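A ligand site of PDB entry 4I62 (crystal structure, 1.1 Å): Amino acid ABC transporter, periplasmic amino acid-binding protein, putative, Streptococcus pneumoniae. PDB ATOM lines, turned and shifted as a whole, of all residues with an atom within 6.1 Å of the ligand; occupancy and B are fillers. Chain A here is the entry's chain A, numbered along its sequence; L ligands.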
ATOM      1  N   LEU A  45      16.062 -18.937   3.780  1.00  0.00           N
ATOM      2  CA  LEU A  45      15.879 -18.567   5.168  1.00  0.00           C
ATOM      3  C   LEU A  45      16.791 -17.386   5.533  1.00  0.00           C
ATOM      4  O   LEU A  45      17.791 -17.132   4.848  1.00  0.00           O
ATOM      5  CB  LEU A  45      16.092 -19.741   6.117  1.00  0.00           C
ATOM      6  CG  LEU A  45      17.527 -20.201   6.352  1.00  0.00           C
ATOM      7  CD1 LEU A  45      17.520 -21.330   7.361  1.00  0.00           C
ATOM      8  CD2 LEU A  45      18.361 -20.571   5.136  1.00  0.00           C
ATOM      9  N   ASN A  46      16.457 -16.718   6.626  1.00  0.00           N
ATOM     10  CA  ASN A  46      17.279 -15.623   7.156  1.00  0.00           C
ATOM     11  C   ASN A  46      17.792 -16.027   8.538  1.00  0.00           C
ATOM     12  O   ASN A  46      17.011 -16.005   9.511  1.00  0.00           O
ATOM     13  CB  ASN A  46      16.436 -14.362   7.241  1.00  0.00           C
ATOM     14  CG  ASN A  46      17.152 -13.263   7.985  1.00  0.00           C
ATOM     15  OD1 ASN A  46      16.667 -12.755   9.018  1.00  0.00           O
ATOM     16  ND2 ASN A  46      18.354 -12.944   7.533  1.00  0.00           N
ATOM     17  N   PRO A  47      19.091 -16.393   8.648  1.00  0.00           N
ATOM     18  CA  PRO A  47      19.580 -17.017   9.890  1.00  0.00           C
ATOM     19  C   PRO A  47      19.991 -16.026  11.015  1.00  0.00           C
ATOM     20  O   PRO A  47      21.137 -15.995  11.469  1.00  0.00           O
ATOM     21  CB  PRO A  47      20.784 -17.826   9.409  1.00  0.00           C
ATOM     22  CG  PRO A  47      21.335 -16.999   8.280  1.00  0.00           C
ATOM     23  CD  PRO A  47      20.096 -16.470   7.574  1.00  0.00           C
ATOM     24  N   ASP A  48      19.031 -15.235  11.481  1.00  0.00           N
ATOM     25  CA  ASP A  48      19.208 -14.279  12.548  1.00  0.00           C
ATOM     26  C   ASP A  48      17.911 -14.319  13.393  1.00  0.00           C
ATOM     27  O   ASP A  48      17.302 -13.264  13.548  1.00  0.00           O
ATOM     28  CB  ASP A  48      19.361 -12.915  11.893  1.00  0.00           C
ATOM     29  CG  ASP A  48      19.792 -11.831  12.864  1.00  0.00           C
ATOM     30  OD1 ASP A  48      20.038 -12.139  14.050  1.00  0.00           O
ATOM     31  OD2 ASP A  48      19.898 -10.664  12.433  1.00  0.00           O
ATOM     32  N   PHE A  49      17.494 -15.504  13.845  1.00  0.00           N
ATOM     33  CA  PHE A  49      16.142 -15.727  14.332  1.00  0.00           C
ATOM     34  C   PHE A  49      16.120 -16.972  15.240  1.00  0.00           C
ATOM     35  O   PHE A  49      15.312 -17.881  15.049  1.00  0.00           O
ATOM     36  CB  PHE A  49      15.177 -15.848  13.134  1.00  0.00           C
ATOM     37  CG  PHE A  49      13.745 -15.521  13.424  1.00  0.00           C
ATOM     38  CD1 PHE A  49      13.372 -14.238  13.734  1.00  0.00           C
ATOM     39  CD2 PHE A  49      12.751 -16.499  13.376  1.00  0.00           C
ATOM     40  CE1 PHE A  49      12.033 -13.918  13.956  1.00  0.00           C
ATOM     41  CE2 PHE A  49      11.429 -16.203  13.598  1.00  0.00           C
ATOM     42  CZ  PHE A  49      11.053 -14.902  13.895  1.00  0.00           C
ATOM     43  N   GLU A  53      16.327 -20.301  13.276  1.00  0.00           N
ATOM     44  CA  GLU A  53      17.561 -20.343  12.466  1.00  0.00           C
ATOM     45  C   GLU A  53      18.482 -19.237  12.960  1.00  0.00           C
ATOM     46  O   GLU A  53      18.038 -18.105  13.153  1.00  0.00           O
ATOM     47  CB  GLU A  53      17.282 -20.191  10.968  1.00  0.00           C
ATOM     48  CG  GLU A  53      16.342 -19.044  10.596  1.00  0.00           C
ATOM     49  CD  GLU A  53      14.885 -19.401  10.661  1.00  0.00           C
ATOM     50  OE1 GLU A  53      14.612 -20.626  10.413  1.00  0.00           O
ATOM     51  OE2 GLU A  53      13.997 -18.533  10.912  1.00  0.00           O
ATOM     52  N   PHE A  90      15.689 -11.455   5.264  1.00  0.00           N
ATOM     53  CA  PHE A  90      14.320 -11.954   5.391  1.00  0.00           C
ATOM     54  C   PHE A  90      13.386 -11.372   4.333  1.00  0.00           C
ATOM     55  O   PHE A  90      12.529 -12.083   3.789  1.00  0.00           O
ATOM     56  CB  PHE A  90      13.729 -11.736   6.773  1.00  0.00           C
ATOM     57  CG  PHE A  90      12.340 -12.341   6.883  1.00  0.00           C
ATOM     58  CD1 PHE A  90      12.201 -13.728   6.953  1.00  0.00           C
ATOM     59  CD2 PHE A  90      11.186 -11.559   6.839  1.00  0.00           C
ATOM     60  CE1 PHE A  90      10.955 -14.293   7.014  1.00  0.00           C
ATOM     61  CE2 PHE A  90       9.953 -12.140   6.891  1.00  0.00           C
ATOM     62  CZ  PHE A  90       9.825 -13.519   7.003  1.00  0.00           C
ATOM     63  N   SER A 107      11.596 -20.448   7.608  1.00  0.00           N
ATOM     64  CA  SER A 107      12.300 -19.298   8.120  1.00  0.00           C
ATOM     65  C   SER A 107      11.441 -18.568   9.153  1.00  0.00           C
ATOM     66  O   SER A 107      11.423 -17.311   9.177  1.00  0.00           O
ATOM     67  CB  SER A 107      12.709 -18.358   6.977  1.00  0.00           C
ATOM     68  OG  SER A 107      13.673 -17.375   7.359  1.00  0.00           O
ATOM     69  N   GLY A 108      10.725 -19.318   9.971  1.00  0.00           N
ATOM     70  CA  GLY A 108       9.825 -18.710  10.940  1.00  0.00           C
ATOM     71  C   GLY A 108       8.742 -17.873  10.256  1.00  0.00           C
ATOM     72  O   GLY A 108       8.360 -16.821  10.772  1.00  0.00           O
ATOM     73  N   VAL A 109       8.225 -18.353   9.132  1.00  0.00           N
ATOM     74  CA  VAL A 109       7.291 -17.596   8.306  1.00  0.00           C
ATOM     75  C   VAL A 109       5.858 -17.712   8.806  1.00  0.00           C
ATOM     76  O   VAL A 109       5.302 -18.839   8.858  1.00  0.00           O
ATOM     77  CB  VAL A 109       7.344 -18.044   6.823  1.00  0.00           C
ATOM     78  CG1 VAL A 109       6.357 -17.269   5.976  1.00  0.00           C
ATOM     79  CG2 VAL A 109       8.731 -17.930   6.271  1.00  0.00           C
ATOM     80  N   SER A 110       5.242 -16.591   9.178  1.00  0.00           N
ATOM     81  CA  SER A 110       3.860 -16.576   9.573  1.00  0.00           C
ATOM     82  C   SER A 110       2.927 -16.681   8.386  1.00  0.00           C
ATOM     83  O   SER A 110       3.083 -16.006   7.347  1.00  0.00           O
ATOM     84  CB  SER A 110       3.572 -15.243  10.246  1.00  0.00           C
ATOM     85  OG  SER A 110       4.378 -15.031  11.407  1.00  0.00           O
ATOM     86  N   LYS A 111       1.853 -17.465   8.533  1.00  0.00           N
ATOM     87  CA  LYS A 111       0.769 -17.402   7.539  1.00  0.00           C
ATOM     88  C   LYS A 111       0.001 -16.096   7.622  1.00  0.00           C
ATOM     89  O   LYS A 111      -0.286 -15.586   8.721  1.00  0.00           O
ATOM     90  CB  LYS A 111      -0.269 -18.471   7.761  1.00  0.00           C
ATOM     91  CG  LYS A 111       0.302 -19.780   7.612  1.00  0.00           C
ATOM     92  CD  LYS A 111      -0.746 -20.879   7.790  1.00  0.00           C
ATOM     93  CE  LYS A 111      -1.897 -20.741   6.824  1.00  0.00           C
ATOM     94  NZ  LYS A 111      -2.958 -21.789   7.106  1.00  0.00           N
ATOM     95  N   ARG A 115      -0.327 -13.435   2.143  1.00  0.00           N
ATOM     96  CA  ARG A 115       0.642 -14.425   1.693  1.00  0.00           C
ATOM     97  C   ARG A 115      -0.027 -15.684   1.116  1.00  0.00           C
ATOM     98  O   ARG A 115       0.495 -16.255   0.159  1.00  0.00           O
ATOM     99  CB  ARG A 115       1.587 -14.777   2.838  1.00  0.00           C
ATOM    100  CG  ARG A 115       2.591 -13.651   3.192  1.00  0.00           C
ATOM    101  CD  ARG A 115       3.325 -13.968   4.495  1.00  0.00           C
ATOM    102  NE  ARG A 115       4.277 -12.908   4.871  1.00  0.00           N
ATOM    103  CZ  ARG A 115       5.046 -12.956   5.930  1.00  0.00           C
ATOM    104  NH1 ARG A 115       4.952 -13.977   6.784  1.00  0.00           N
ATOM    105  NH2 ARG A 115       5.918 -11.957   6.165  1.00  0.00           N
ATOM    106  N   GLN A 156      11.490  -5.850  11.940  1.00  0.00           N
ATOM    107  CA  GLN A 156      12.264  -6.335  10.796  1.00  0.00           C
ATOM    108  C   GLN A 156      11.540  -6.044   9.485  1.00  0.00           C
ATOM    109  O   GLN A 156      10.339  -6.317   9.319  1.00  0.00           O
ATOM    110  CB  GLN A 156      12.575  -7.831  10.926  1.00  0.00           C
ATOM    111  CG  GLN A 156      13.456  -8.310   9.740  1.00  0.00           C
ATOM    112  CD  GLN A 156      13.970  -9.742   9.847  1.00  0.00           C
ATOM    113  OE1 GLN A 156      13.217 -10.650  10.171  1.00  0.00           O
ATOM    114  NE2 GLN A 156      15.225  -9.947   9.548  1.00  0.00           N
ATOM    115  N   GLY A 158       9.949  -6.443   6.061  1.00  0.00           N
ATOM    116  CA  GLY A 158       9.330  -7.595   5.407  1.00  0.00           C
ATOM    117  C   GLY A 158       8.557  -8.488   6.362  1.00  0.00           C
ATOM    118  O   GLY A 158       7.956  -9.470   5.899  1.00  0.00           O
ATOM    119  N   SER A 159       8.567  -8.178   7.649  1.00  0.00           N
ATOM    120  CA  SER A 159       7.898  -9.046   8.630  1.00  0.00           C
ATOM    121  C   SER A 159       6.463  -8.606   8.905  1.00  0.00           C
ATOM    122  O   SER A 159       6.093  -7.433   8.696  1.00  0.00           O
ATOM    123  CB  SER A 159       8.673  -9.052   9.949  1.00  0.00           C
ATOM    124  OG  SER A 159       8.545  -7.812  10.646  1.00  0.00           O
ATOM    125  N   ILE A 160       5.664  -9.517   9.469  1.00  0.00           N
ATOM    126  CA  ILE A 160       4.340  -9.140   9.889  1.00  0.00           C
ATOM    127  C   ILE A 160       4.376  -8.183  11.082  1.00  0.00           C
ATOM    128  O   ILE A 160       3.410  -7.446  11.328  1.00  0.00           O
ATOM    129  CB  ILE A 160       3.421 -10.350  10.160  1.00  0.00           C
ATOM    130  CG1 ILE A 160       3.832 -11.138  11.397  1.00  0.00           C
ATOM    131  CG2 ILE A 160       3.353 -11.292   8.955  1.00  0.00           C
ATOM    132  CD1 ILE A 160       2.719 -12.002  11.944  1.00  0.00           C
ATOM    133  N   GLN A 161       5.471  -8.168  11.809  1.00  0.00           N
ATOM    134  CA  GLN A 161       5.641  -7.205  12.896  1.00  0.00           C
ATOM    135  C   GLN A 161       5.737  -5.792  12.342  1.00  0.00           C
ATOM    136  O   GLN A 161       5.193  -4.849  12.953  1.00  0.00           O
ATOM    137  CB  GLN A 161       6.893  -7.551  13.715  1.00  0.00           C
ATOM    138  CG  GLN A 161       6.734  -8.803  14.597  1.00  0.00           C
ATOM    139  CD  GLN A 161       6.607 -10.092  13.808  1.00  0.00           C
ATOM    140  OE1 GLN A 161       7.273 -10.310  12.787  1.00  0.00           O
ATOM    141  NE2 GLN A 161       5.743 -10.978  14.283  1.00  0.00           N
ATOM    142  N   ASN A 180      17.858  -8.367  12.019  1.00  0.00           N
ATOM    143  CA  ASN A 180      17.463  -8.375  13.438  1.00  0.00           C
ATOM    144  C   ASN A 180      18.580  -7.926  14.353  1.00  0.00           C
ATOM    145  O   ASN A 180      18.336  -7.246  15.366  1.00  0.00           O
ATOM    146  CB  ASN A 180      16.935  -9.738  13.838  1.00  0.00           C
ATOM    147  CG  ASN A 180      15.626 -10.060  13.168  1.00  0.00           C
ATOM    148  OD1 ASN A 180      14.756  -9.181  13.015  1.00  0.00           O
ATOM    149  ND2 ASN A 180      15.423 -11.322  12.793  1.00  0.00           N
ATOM    150  N   GLU A 198       8.310 -11.877  17.973  1.00  0.00           N
ATOM    151  CA  GLU A 198       7.596 -13.025  18.514  1.00  0.00           C
ATOM    152  C   GLU A 198       8.319 -13.565  19.757  1.00  0.00           C
ATOM    153  O   GLU A 198       9.549 -13.544  19.829  1.00  0.00           O
ATOM    154  CB  GLU A 198       7.414 -14.079  17.428  1.00  0.00           C
ATOM    155  CG  GLU A 198       6.338 -13.599  16.420  1.00  0.00           C
ATOM    156  CD  GLU A 198       6.536 -14.002  14.954  1.00  0.00           C
ATOM    157  OE1 GLU A 198       7.684 -14.260  14.510  1.00  0.00           O
ATOM    158  OE2 GLU A 198       5.534 -13.959  14.208  1.00  0.00           O
ATOM    159  N   ASP A 225      -1.108 -16.274  14.951  1.00  0.00           N
ATOM    160  CA  ASP A 225       0.186 -16.114  14.331  1.00  0.00           C
ATOM    161  C   ASP A 225       0.825 -17.490  14.312  1.00  0.00           C
ATOM    162  O   ASP A 225       1.459 -17.904  15.307  1.00  0.00           O
ATOM    163  CB  ASP A 225       1.023 -15.130  15.146  1.00  0.00           C
ATOM    164  CG  ASP A 225       2.377 -14.857  14.522  1.00  0.00           C
ATOM    165  OD1 ASP A 225       2.683 -15.411  13.435  1.00  0.00           O
ATOM    166  OD2 ASP A 225       3.129 -14.064  15.128  1.00  0.00           O
ATOM    167  N   TYR A 227       3.365 -20.296  12.355  1.00  0.00           N
ATOM    168  CA  TYR A 227       4.428 -20.495  11.396  1.00  0.00           C
ATOM    169  C   TYR A 227       4.124 -21.704  10.507  1.00  0.00           C
ATOM    170  O   TYR A 227       3.577 -22.712  10.959  1.00  0.00           O
ATOM    171  CB  TYR A 227       5.763 -20.776  12.085  1.00  0.00           C
ATOM    172  CG  TYR A 227       6.390 -19.695  12.881  1.00  0.00           C
ATOM    173  CD1 TYR A 227       5.871 -18.420  12.946  1.00  0.00           C
ATOM    174  CD2 TYR A 227       7.552 -19.992  13.604  1.00  0.00           C
ATOM    175  CE1 TYR A 227       6.505 -17.418  13.727  1.00  0.00           C
ATOM    176  CE2 TYR A 227       8.180 -19.023  14.378  1.00  0.00           C
ATOM    177  CZ  TYR A 227       7.652 -17.757  14.438  1.00  0.00           C
ATOM    178  OH  TYR A 227       8.339 -16.824  15.202  1.00  0.00           O
HETATM  179  N1  LIG L   1       7.112 -14.454  11.657  1.00  0.00           N
HETATM  180  C1  LIG L   1       7.460 -13.169  10.993  1.00  0.00           C
HETATM  181  C2  LIG L   1       6.983 -13.149   9.544  1.00  0.00           C
HETATM  182  O1  LIG L   1       6.720 -14.225   8.972  1.00  0.00           O
HETATM  183  C3  LIG L   1       8.939 -12.862  11.125  1.00  0.00           C
HETATM  184  C4  LIG L   1       9.847 -13.973  10.602  1.00  0.00           C
HETATM  185  C5  LIG L   1      11.290 -13.532  10.478  1.00  0.00           C
HETATM  186  N2  LIG L   1      12.146 -14.679  10.269  1.00  0.00           N
HETATM  187  C6  LIG L   1      13.448 -14.628  10.102  1.00  0.00           C
HETATM  188  N3  LIG L   1      14.133 -15.752   9.910  1.00  0.00           N
HETATM  189  N4  LIG L   1      14.079 -13.460  10.116  1.00  0.00           N
HETATM  190  O2  LIG L   1       6.922 -12.008   8.982  1.00  0.00           O
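OE1 of Gln 156 lies within hydrogen-bond range of N4 of the ligand. The backbone NH (N) of Ser 110 sits at hydrogen-bond distance from an oxygen (O1) of the ligand (2.8 Å). The side-chain carboxylate (OE1) of Glu 198 lies within salt-bridge range of a nitrogen (N1) of the ligand (2.9 Å). The backbone carbonyl oxygen of Gly 108 lies within hydrogen-bond range of a nitrogen (N1) of the ligand (2.8 Å). N2 of the ligand sits at hydrogen-bond distance from O of Ser 107. N of Ile 160 sits at hydrogen-bond distance from O2 of the ligand (2.8 Å). The side-chain amide oxygen (OD1) of Asn 46 sits at hydrogen-bond distance from a nitrogen (N4) of the ligand (2.9 Å). A nitrogen (N3) of the ligand lies within hydrogen-bond range of the side-chain hydroxyl (OG) of Ser 107 (3.1 Å). OE2 of Glu 53 lies within salt-bridge range of N3 of the ligand, 3.0 Å away. A nitrogen (N1) of the ligand is in hydrogen-bond range of the side-chain hydroxyl (OG) of Ser 110. An oxygen (O1) of the ligand lies within salt-bridge range of the guanidinium group (NH1) of Arg 115 (2.8 Å). The backbone carbonyl oxygen (O) of Asn 46 is in hydrogen-bond range of a nitrogen (N3) of the ligand (2.9 Å).
Merely in contact with the ligand: Ser 159, Gln 161, Phe 49, Phe 90, Val 109, Tyr 227 and Asn 180. Hydrophobic or aromatic side chains within 4 Å of the ligand: Phe 49, Phe 90, Ile 160 and Tyr 227. Within 4 Å of the ligand: Asn 46, Phe 49, Glu 53, Phe 90, Ser 107, Gly 108, Val 109, Ser 110, Arg 115, Gln 156, Ser 159, Ile 160, Gln 161, Asn 180, Glu 198 and Tyr 227.
OG of Ser 159 sits close to N of Gln 161, at 3.3 Å. The guanidinium group (NH1) of Arg 115 lies within hydrogen-bond range of the backbone carbonyl oxygen (O) of Ser 110, at 2.8 Å. The backbone carbonyl oxygen (O) of Gln 156 lies within hydrogen-bond range of the side-chain hydroxyl (OG) of Ser 159 (2.7 Å). O of Asp 48 lies within hydrogen-bond range of ND2 of Asn 180 (2.8 Å). The side-chain carboxylate of Glu 198 is in hydrogen-bond range of the side-chain hydroxyl of Tyr 227 (2.7 Å). OE2 of Glu 198 lies close to OD2 of Asp 225 (2.6 Å). OG of Ser 107 lies within hydrogen-bond range of N of Asn 46 (3.0 Å). NE2 of Gln 156 sits at hydrogen-bond distance from OD1 of Asn 46 (3.2 Å).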
